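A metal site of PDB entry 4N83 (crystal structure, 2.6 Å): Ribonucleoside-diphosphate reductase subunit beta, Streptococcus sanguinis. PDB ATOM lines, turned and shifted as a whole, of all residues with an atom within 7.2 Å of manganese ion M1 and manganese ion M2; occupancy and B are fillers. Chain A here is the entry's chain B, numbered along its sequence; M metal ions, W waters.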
ATOM      1  N   LEU A  62      -7.084  29.230  -7.794  1.00  0.00           N
ATOM      2  CA  LEU A  62      -8.229  28.712  -8.516  1.00  0.00           C
ATOM      3  C   LEU A  62      -8.944  27.609  -7.725  1.00  0.00           C
ATOM      4  O   LEU A  62     -10.170  27.500  -7.782  1.00  0.00           O
ATOM      5  CB  LEU A  62      -7.786  28.204  -9.902  1.00  0.00           C
ATOM      6  CG  LEU A  62      -7.193  29.264 -10.845  1.00  0.00           C
ATOM      7  CD1 LEU A  62      -6.395  28.610 -11.969  1.00  0.00           C
ATOM      8  CD2 LEU A  62      -8.266  30.168 -11.445  1.00  0.00           C
ATOM      9  N   LEU A  65     -11.499  29.013  -5.154  1.00  0.00           N
ATOM     10  CA  LEU A  65     -12.696  29.656  -5.663  1.00  0.00           C
ATOM     11  C   LEU A  65     -13.641  28.674  -6.312  1.00  0.00           C
ATOM     12  O   LEU A  65     -14.857  28.836  -6.224  1.00  0.00           O
ATOM     13  CB  LEU A  65     -12.316  30.747  -6.663  1.00  0.00           C
ATOM     14  CG  LEU A  65     -11.456  31.850  -6.018  1.00  0.00           C
ATOM     15  CD1 LEU A  65     -10.651  32.570  -7.090  1.00  0.00           C
ATOM     16  CD2 LEU A  65     -12.318  32.802  -5.204  1.00  0.00           C
ATOM     17  N   ASP A  66     -13.095  27.671  -6.995  1.00  0.00           N
ATOM     18  CA  ASP A  66     -13.897  26.542  -7.457  1.00  0.00           C
ATOM     19  C   ASP A  66     -14.432  25.738  -6.266  1.00  0.00           C
ATOM     20  O   ASP A  66     -15.534  25.191  -6.341  1.00  0.00           O
ATOM     21  CB  ASP A  66     -13.109  25.632  -8.413  1.00  0.00           C
ATOM     22  CG  ASP A  66     -13.393  25.942  -9.887  1.00  0.00           C
ATOM     23  OD1 ASP A  66     -14.541  26.313 -10.201  1.00  0.00           O
ATOM     24  OD2 ASP A  66     -12.475  25.784 -10.730  1.00  0.00           O
ATOM     25  N   THR A  67     -13.663  25.680  -5.176  1.00  0.00           N
ATOM     26  CA  THR A  67     -14.168  25.131  -3.910  1.00  0.00           C
ATOM     27  C   THR A  67     -15.369  25.945  -3.460  1.00  0.00           C
ATOM     28  O   THR A  67     -16.421  25.391  -3.163  1.00  0.00           O
ATOM     29  CB  THR A  67     -13.070  25.108  -2.810  1.00  0.00           C
ATOM     30  OG1 THR A  67     -12.050  24.179  -3.154  1.00  0.00           O
ATOM     31  CG2 THR A  67     -13.639  24.715  -1.457  1.00  0.00           C
ATOM     32  N   GLN A  69     -17.372  27.739  -5.230  1.00  0.00           N
ATOM     33  CA  GLN A  69     -18.471  27.536  -6.166  1.00  0.00           C
ATOM     34  C   GLN A  69     -19.217  26.209  -5.963  1.00  0.00           C
ATOM     35  O   GLN A  69     -20.415  26.126  -6.221  1.00  0.00           O
ATOM     36  CB  GLN A  69     -17.952  27.596  -7.601  1.00  0.00           C
ATOM     37  CG  GLN A  69     -17.511  28.995  -8.039  1.00  0.00           C
ATOM     38  CD  GLN A  69     -18.660  29.984  -8.100  1.00  0.00           C
ATOM     39  OE1 GLN A  69     -19.122  30.474  -7.063  1.00  0.00           O
ATOM     40  NE2 GLN A  69     -19.098  30.305  -9.306  1.00  0.00           N
ATOM     41  N   SER A  70     -18.501  25.182  -5.505  1.00  0.00           N
ATOM     42  CA  SER A  70     -19.064  23.859  -5.333  1.00  0.00           C
ATOM     43  C   SER A  70     -19.794  23.708  -3.999  1.00  0.00           C
ATOM     44  O   SER A  70     -20.615  22.796  -3.846  1.00  0.00           O
ATOM     45  CB  SER A  70     -17.939  22.827  -5.414  1.00  0.00           C
ATOM     46  OG  SER A  70     -17.113  22.910  -4.260  1.00  0.00           O
ATOM     47  N   VAL A  74     -23.152  27.665  -6.085  1.00  0.00           N
ATOM     48  CA  VAL A  74     -24.316  27.098  -6.772  1.00  0.00           C
ATOM     49  C   VAL A  74     -25.475  26.880  -5.811  1.00  0.00           C
ATOM     50  O   VAL A  74     -26.640  26.962  -6.202  1.00  0.00           O
ATOM     51  CB  VAL A  74     -23.956  25.765  -7.478  1.00  0.00           C
ATOM     52  CG1 VAL A  74     -25.201  25.142  -8.094  1.00  0.00           C
ATOM     53  CG2 VAL A  74     -22.902  25.997  -8.546  1.00  0.00           C
ATOM     54  N   ILE A  93     -24.021  21.571 -12.681  1.00  0.00           N
ATOM     55  CA  ILE A  93     -23.016  22.619 -12.485  1.00  0.00           C
ATOM     56  C   ILE A  93     -22.315  22.432 -11.137  1.00  0.00           C
ATOM     57  O   ILE A  93     -21.096  22.433 -11.076  1.00  0.00           O
ATOM     58  CB  ILE A  93     -23.629  24.033 -12.611  1.00  0.00           C
ATOM     59  CG1 ILE A  93     -24.027  24.316 -14.062  1.00  0.00           C
ATOM     60  CG2 ILE A  93     -22.638  25.088 -12.144  1.00  0.00           C
ATOM     61  CD1 ILE A  93     -24.987  25.466 -14.254  1.00  0.00           C
ATOM     62  N   MET A  96     -19.913  19.578 -11.259  1.00  0.00           N
ATOM     63  CA  MET A  96     -18.743  19.855 -12.091  1.00  0.00           C
ATOM     64  C   MET A  96     -17.788  20.862 -11.459  1.00  0.00           C
ATOM     65  O   MET A  96     -16.614  20.845 -11.791  1.00  0.00           O
ATOM     66  CB  MET A  96     -19.167  20.307 -13.485  1.00  0.00           C
ATOM     67  CG  MET A  96     -19.856  19.204 -14.281  1.00  0.00           C
ATOM     68  SD  MET A  96     -18.941  17.653 -14.418  1.00  0.00           S
ATOM     69  CE  MET A  96     -17.532  18.119 -15.417  1.00  0.00           C
ATOM     70  N   GLU A  97     -18.280  21.693 -10.546  1.00  0.00           N
ATOM     71  CA  GLU A  97     -17.417  22.567  -9.767  1.00  0.00           C
ATOM     72  C   GLU A  97     -16.525  21.767  -8.813  1.00  0.00           C
ATOM     73  O   GLU A  97     -15.378  22.157  -8.550  1.00  0.00           O
ATOM     74  CB  GLU A  97     -18.218  23.587  -8.967  1.00  0.00           C
ATOM     75  CG  GLU A  97     -19.038  24.580  -9.771  1.00  0.00           C
ATOM     76  CD  GLU A  97     -18.225  25.456 -10.699  1.00  0.00           C
ATOM     77  OE1 GLU A  97     -16.990  25.305 -10.762  1.00  0.00           O
ATOM     78  OE2 GLU A  97     -18.842  26.299 -11.378  1.00  0.00           O
ATOM     79  N   SER A  98     -17.052  20.659  -8.278  1.00  0.00           N
ATOM     80  CA  SER A  98     -16.256  19.741  -7.457  1.00  0.00           C
ATOM     81  C   SER A  98     -15.194  19.010  -8.274  1.00  0.00           C
ATOM     82  O   SER A  98     -14.109  18.732  -7.780  1.00  0.00           O
ATOM     83  CB  SER A  98     -17.151  18.741  -6.713  1.00  0.00           C
ATOM     84  OG  SER A  98     -17.745  19.349  -5.579  1.00  0.00           O
ATOM     85  N   HIS A 100     -13.868  20.401 -10.879  1.00  0.00           N
ATOM     86  CA  HIS A 100     -12.925  21.477 -11.146  1.00  0.00           C
ATOM     87  C   HIS A 100     -11.939  21.607  -9.987  1.00  0.00           C
ATOM     88  O   HIS A 100     -10.727  21.541 -10.188  1.00  0.00           O
ATOM     89  CB  HIS A 100     -13.651  22.811 -11.374  1.00  0.00           C
ATOM     90  CG  HIS A 100     -14.458  22.852 -12.630  1.00  0.00           C
ATOM     91  ND1 HIS A 100     -15.424  23.801 -12.857  1.00  0.00           N
ATOM     92  CD2 HIS A 100     -14.445  22.057 -13.719  1.00  0.00           C
ATOM     93  CE1 HIS A 100     -15.964  23.595 -14.052  1.00  0.00           C
ATOM     94  NE2 HIS A 100     -15.384  22.542 -14.587  1.00  0.00           N
ATOM     95  N   ALA A 101     -12.479  21.783  -8.787  1.00  0.00           N
ATOM     96  CA  ALA A 101     -11.674  21.892  -7.574  1.00  0.00           C
ATOM     97  C   ALA A 101     -10.706  20.723  -7.444  1.00  0.00           C
ATOM     98  O   ALA A 101      -9.513  20.917  -7.206  1.00  0.00           O
ATOM     99  CB  ALA A 101     -12.575  21.977  -6.354  1.00  0.00           C
ATOM    100  N   TYR A 104      -7.363  20.241  -9.828  1.00  0.00           N
ATOM    101  CA  TYR A 104      -6.153  20.933  -9.381  1.00  0.00           C
ATOM    102  C   TYR A 104      -5.319  20.047  -8.482  1.00  0.00           C
ATOM    103  O   TYR A 104      -4.086  20.089  -8.544  1.00  0.00           O
ATOM    104  CB  TYR A 104      -6.511  22.234  -8.655  1.00  0.00           C
ATOM    105  CG  TYR A 104      -7.354  23.181  -9.486  1.00  0.00           C
ATOM    106  CD1 TYR A 104      -6.902  23.638 -10.722  1.00  0.00           C
ATOM    107  CD2 TYR A 104      -8.595  23.623  -9.043  1.00  0.00           C
ATOM    108  CE1 TYR A 104      -7.670  24.497 -11.485  1.00  0.00           C
ATOM    109  CE2 TYR A 104      -9.368  24.488  -9.800  1.00  0.00           C
ATOM    110  CZ  TYR A 104      -8.902  24.915 -11.024  1.00  0.00           C
ATOM    111  OH  TYR A 104      -9.653  25.774 -11.788  1.00  0.00           O
ATOM    112  N   SER A 153     -21.483  35.458  -9.505  1.00  0.00           N
ATOM    113  CA  SER A 153     -21.003  34.168 -10.005  1.00  0.00           C
ATOM    114  C   SER A 153     -20.446  34.293 -11.436  1.00  0.00           C
ATOM    115  O   SER A 153     -19.521  33.574 -11.804  1.00  0.00           O
ATOM    116  CB  SER A 153     -22.109  33.114  -9.952  1.00  0.00           C
ATOM    117  OG  SER A 153     -21.620  31.856 -10.390  1.00  0.00           O
ATOM    118  N   GLU A 157     -16.256  33.667 -12.534  1.00  0.00           N
ATOM    119  CA  GLU A 157     -15.751  32.583 -13.388  1.00  0.00           C
ATOM    120  C   GLU A 157     -15.673  32.906 -14.882  1.00  0.00           C
ATOM    121  O   GLU A 157     -15.105  32.134 -15.654  1.00  0.00           O
ATOM    122  CB  GLU A 157     -16.537  31.300 -13.146  1.00  0.00           C
ATOM    123  CG  GLU A 157     -16.037  30.528 -11.935  1.00  0.00           C
ATOM    124  CD  GLU A 157     -16.783  29.235 -11.714  1.00  0.00           C
ATOM    125  OE1 GLU A 157     -18.022  29.265 -11.612  1.00  0.00           O
ATOM    126  OE2 GLU A 157     -16.122  28.174 -11.643  1.00  0.00           O
ATOM    127  N   PHE A 161     -11.416  34.612 -12.818  1.00  0.00           N
ATOM    128  CA  PHE A 161     -10.621  33.378 -12.943  1.00  0.00           C
ATOM    129  C   PHE A 161      -9.473  33.509 -13.946  1.00  0.00           C
ATOM    130  O   PHE A 161      -8.488  32.751 -13.877  1.00  0.00           O
ATOM    131  CB  PHE A 161     -11.491  32.176 -13.321  1.00  0.00           C
ATOM    132  CG  PHE A 161     -11.881  31.302 -12.154  1.00  0.00           C
ATOM    133  CD1 PHE A 161     -11.484  29.979 -12.100  1.00  0.00           C
ATOM    134  CD2 PHE A 161     -12.656  31.804 -11.109  1.00  0.00           C
ATOM    135  CE1 PHE A 161     -11.847  29.171 -11.036  1.00  0.00           C
ATOM    136  CE2 PHE A 161     -13.019  30.997 -10.045  1.00  0.00           C
ATOM    137  CZ  PHE A 161     -12.617  29.677 -10.007  1.00  0.00           C
ATOM    138  N   PHE A 165      -6.080  31.757 -15.302  1.00  0.00           N
ATOM    139  CA  PHE A 165      -6.022  30.950 -16.533  1.00  0.00           C
ATOM    140  C   PHE A 165      -4.979  31.435 -17.532  1.00  0.00           C
ATOM    141  O   PHE A 165      -4.512  30.655 -18.365  1.00  0.00           O
ATOM    142  CB  PHE A 165      -7.390  30.888 -17.232  1.00  0.00           C
ATOM    143  CG  PHE A 165      -8.449  30.090 -16.484  1.00  0.00           C
ATOM    144  CD1 PHE A 165      -8.130  28.946 -15.759  1.00  0.00           C
ATOM    145  CD2 PHE A 165      -9.786  30.469 -16.566  1.00  0.00           C
ATOM    146  CE1 PHE A 165      -9.115  28.229 -15.098  1.00  0.00           C
ATOM    147  CE2 PHE A 165     -10.771  29.747 -15.918  1.00  0.00           C
ATOM    148  CZ  PHE A 165     -10.442  28.624 -15.186  1.00  0.00           C
ATOM    149  N   ILE A 187     -12.099  22.892 -18.080  1.00  0.00           N
ATOM    150  CA  ILE A 187     -12.731  23.741 -17.077  1.00  0.00           C
ATOM    151  C   ILE A 187     -13.334  24.971 -17.754  1.00  0.00           C
ATOM    152  O   ILE A 187     -14.452  25.365 -17.441  1.00  0.00           O
ATOM    153  CB  ILE A 187     -11.720  24.192 -15.997  1.00  0.00           C
ATOM    154  CG1 ILE A 187     -11.278  22.984 -15.161  1.00  0.00           C
ATOM    155  CG2 ILE A 187     -12.333  25.275 -15.107  1.00  0.00           C
ATOM    156  CD1 ILE A 187     -10.268  23.292 -14.087  1.00  0.00           C
ATOM    157  N   ASP A 190     -16.546  24.327 -19.614  1.00  0.00           N
ATOM    158  CA  ASP A 190     -17.704  24.285 -18.721  1.00  0.00           C
ATOM    159  C   ASP A 190     -18.089  25.692 -18.308  1.00  0.00           C
ATOM    160  O   ASP A 190     -19.266  26.046 -18.342  1.00  0.00           O
ATOM    161  CB  ASP A 190     -17.407  23.437 -17.473  1.00  0.00           C
ATOM    162  CG  ASP A 190     -17.211  21.968 -17.792  1.00  0.00           C
ATOM    163  OD1 ASP A 190     -17.684  21.528 -18.854  1.00  0.00           O
ATOM    164  OD2 ASP A 190     -16.579  21.267 -16.964  1.00  0.00           O
ATOM    165  N   GLU A 191     -17.099  26.487 -17.914  1.00  0.00           N
ATOM    166  CA  GLU A 191     -17.347  27.827 -17.375  1.00  0.00           C
ATOM    167  C   GLU A 191     -17.926  28.819 -18.402  1.00  0.00           C
ATOM    168  O   GLU A 191     -18.597  29.771 -18.013  1.00  0.00           O
ATOM    169  CB  GLU A 191     -16.087  28.403 -16.726  1.00  0.00           C
ATOM    170  CG  GLU A 191     -15.638  27.686 -15.466  1.00  0.00           C
ATOM    171  CD  GLU A 191     -16.761  27.499 -14.466  1.00  0.00           C
ATOM    172  OE1 GLU A 191     -17.637  28.397 -14.359  1.00  0.00           O
ATOM    173  OE2 GLU A 191     -16.790  26.460 -13.782  1.00  0.00           O
ATOM    174  N   SER A 192     -17.667  28.620 -19.687  1.00  0.00           N
ATOM    175  CA  SER A 192     -18.230  29.489 -20.705  1.00  0.00           C
ATOM    176  C   SER A 192     -19.744  29.273 -20.814  1.00  0.00           C
ATOM    177  O   SER A 192     -20.514  30.237 -20.927  1.00  0.00           O
ATOM    178  CB  SER A 192     -17.542  29.299 -22.064  1.00  0.00           C
ATOM    179  OG  SER A 192     -17.737  27.988 -22.550  1.00  0.00           O
ATOM    180  N   HIS A 194     -21.517  27.877 -18.339  1.00  0.00           N
ATOM    181  CA  HIS A 194     -22.002  28.308 -17.021  1.00  0.00           C
ATOM    182  C   HIS A 194     -22.384  29.787 -17.015  1.00  0.00           C
ATOM    183  O   HIS A 194     -23.464  30.156 -16.543  1.00  0.00           O
ATOM    184  CB  HIS A 194     -20.942  28.036 -15.937  1.00  0.00           C
ATOM    185  CG  HIS A 194     -20.718  26.585 -15.643  1.00  0.00           C
ATOM    186  ND1 HIS A 194     -19.921  26.155 -14.600  1.00  0.00           N
ATOM    187  CD2 HIS A 194     -21.198  25.463 -16.235  1.00  0.00           C
ATOM    188  CE1 HIS A 194     -19.903  24.829 -14.589  1.00  0.00           C
ATOM    189  NE2 HIS A 194     -20.671  24.383 -15.567  1.00  0.00           N
ATOM    190  N   GLY A 195     -21.506  30.631 -17.546  1.00  0.00           N
ATOM    191  CA  GLY A 195     -21.718  32.071 -17.541  1.00  0.00           C
ATOM    192  C   GLY A 195     -22.806  32.516 -18.501  1.00  0.00           C
ATOM    193  O   GLY A 195     -23.589  33.412 -18.184  1.00  0.00           O
ATOM    194  N   ILE A 198     -26.123  31.329 -16.701  1.00  0.00           N
ATOM    195  CA  ILE A 198     -26.447  32.170 -15.548  1.00  0.00           C
ATOM    196  C   ILE A 198     -26.765  33.593 -16.002  1.00  0.00           C
ATOM    197  O   ILE A 198     -27.642  34.247 -15.436  1.00  0.00           O
ATOM    198  CB  ILE A 198     -25.302  32.202 -14.517  1.00  0.00           C
ATOM    199  CG1 ILE A 198     -25.053  30.814 -13.937  1.00  0.00           C
ATOM    200  CG2 ILE A 198     -25.636  33.160 -13.378  1.00  0.00           C
ATOM    201  CD1 ILE A 198     -23.712  30.681 -13.230  1.00  0.00           C
HETATM  202 MN    MN M   1     -15.514  25.991 -11.955  1.00  0.00          MN
HETATM  203 MN    MN M   2     -18.895  27.515 -12.787  1.00  0.00          MN
HETATM  204  O   HOH W   1     -20.665  28.868 -12.036  1.00  0.00           O
HETATM  205  O   HOH W   2     -13.556  27.202 -12.909  1.00  0.00           O
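Manganese ion M2 is bound by the side-chain carboxylate (OE2) of Glu 97, the side-chain carboxylate (OE1) of Glu 191, the side-chain carboxylate (OE1) of Glu 157, water W1, a ring nitrogen (ND1) of His 194 and the side-chain carboxylate (OE2) of Glu 191.
Manganese ion M2 has six donor atoms within binding distance.
OD2 of Asp 66 sits at hydrogen-bond distance from OH of Tyr 104.
The backbone carbonyl oxygen (O) of Asp 66 is in hydrogen-bond range of the side-chain hydroxyl (OG) of Ser 70 (3.5 Å).
The side-chain carboxylate (OE1) of Glu 157 sits close to the side-chain amide nitrogen (NE2) of Gln 69 (2.7 Å).
The backbone carbonyl oxygen (O) of Met 96 sits close to a ring nitrogen (NE2) of His 100, at 3.5 Å.
NE2 of His 100 is in hydrogen-bond range of OD2 of Asp 190, 3.0 Å away.
Within 4 Å of manganese ion M2: Glu 97, Glu 157, Glu 191 and His 194.
Of the 25 residues printed, 5 come within 4 Å of manganese ion M1.
The nearest printed residue that does not touch manganese ion M1 is Ile 187 (4.5 Å).
Manganese ion M1 is bound by OE1 of Glu 97 (2.0 Å), OD1 of Asp 66 (2.0 Å), OE2 of Glu 191 (2.3 Å), OE2 of Glu 157 (2.3 Å), ND1 of His 100 (2.4 Å) and water W2 (2.5 Å).
Manganese ion M1 has six donor atoms within binding distance.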
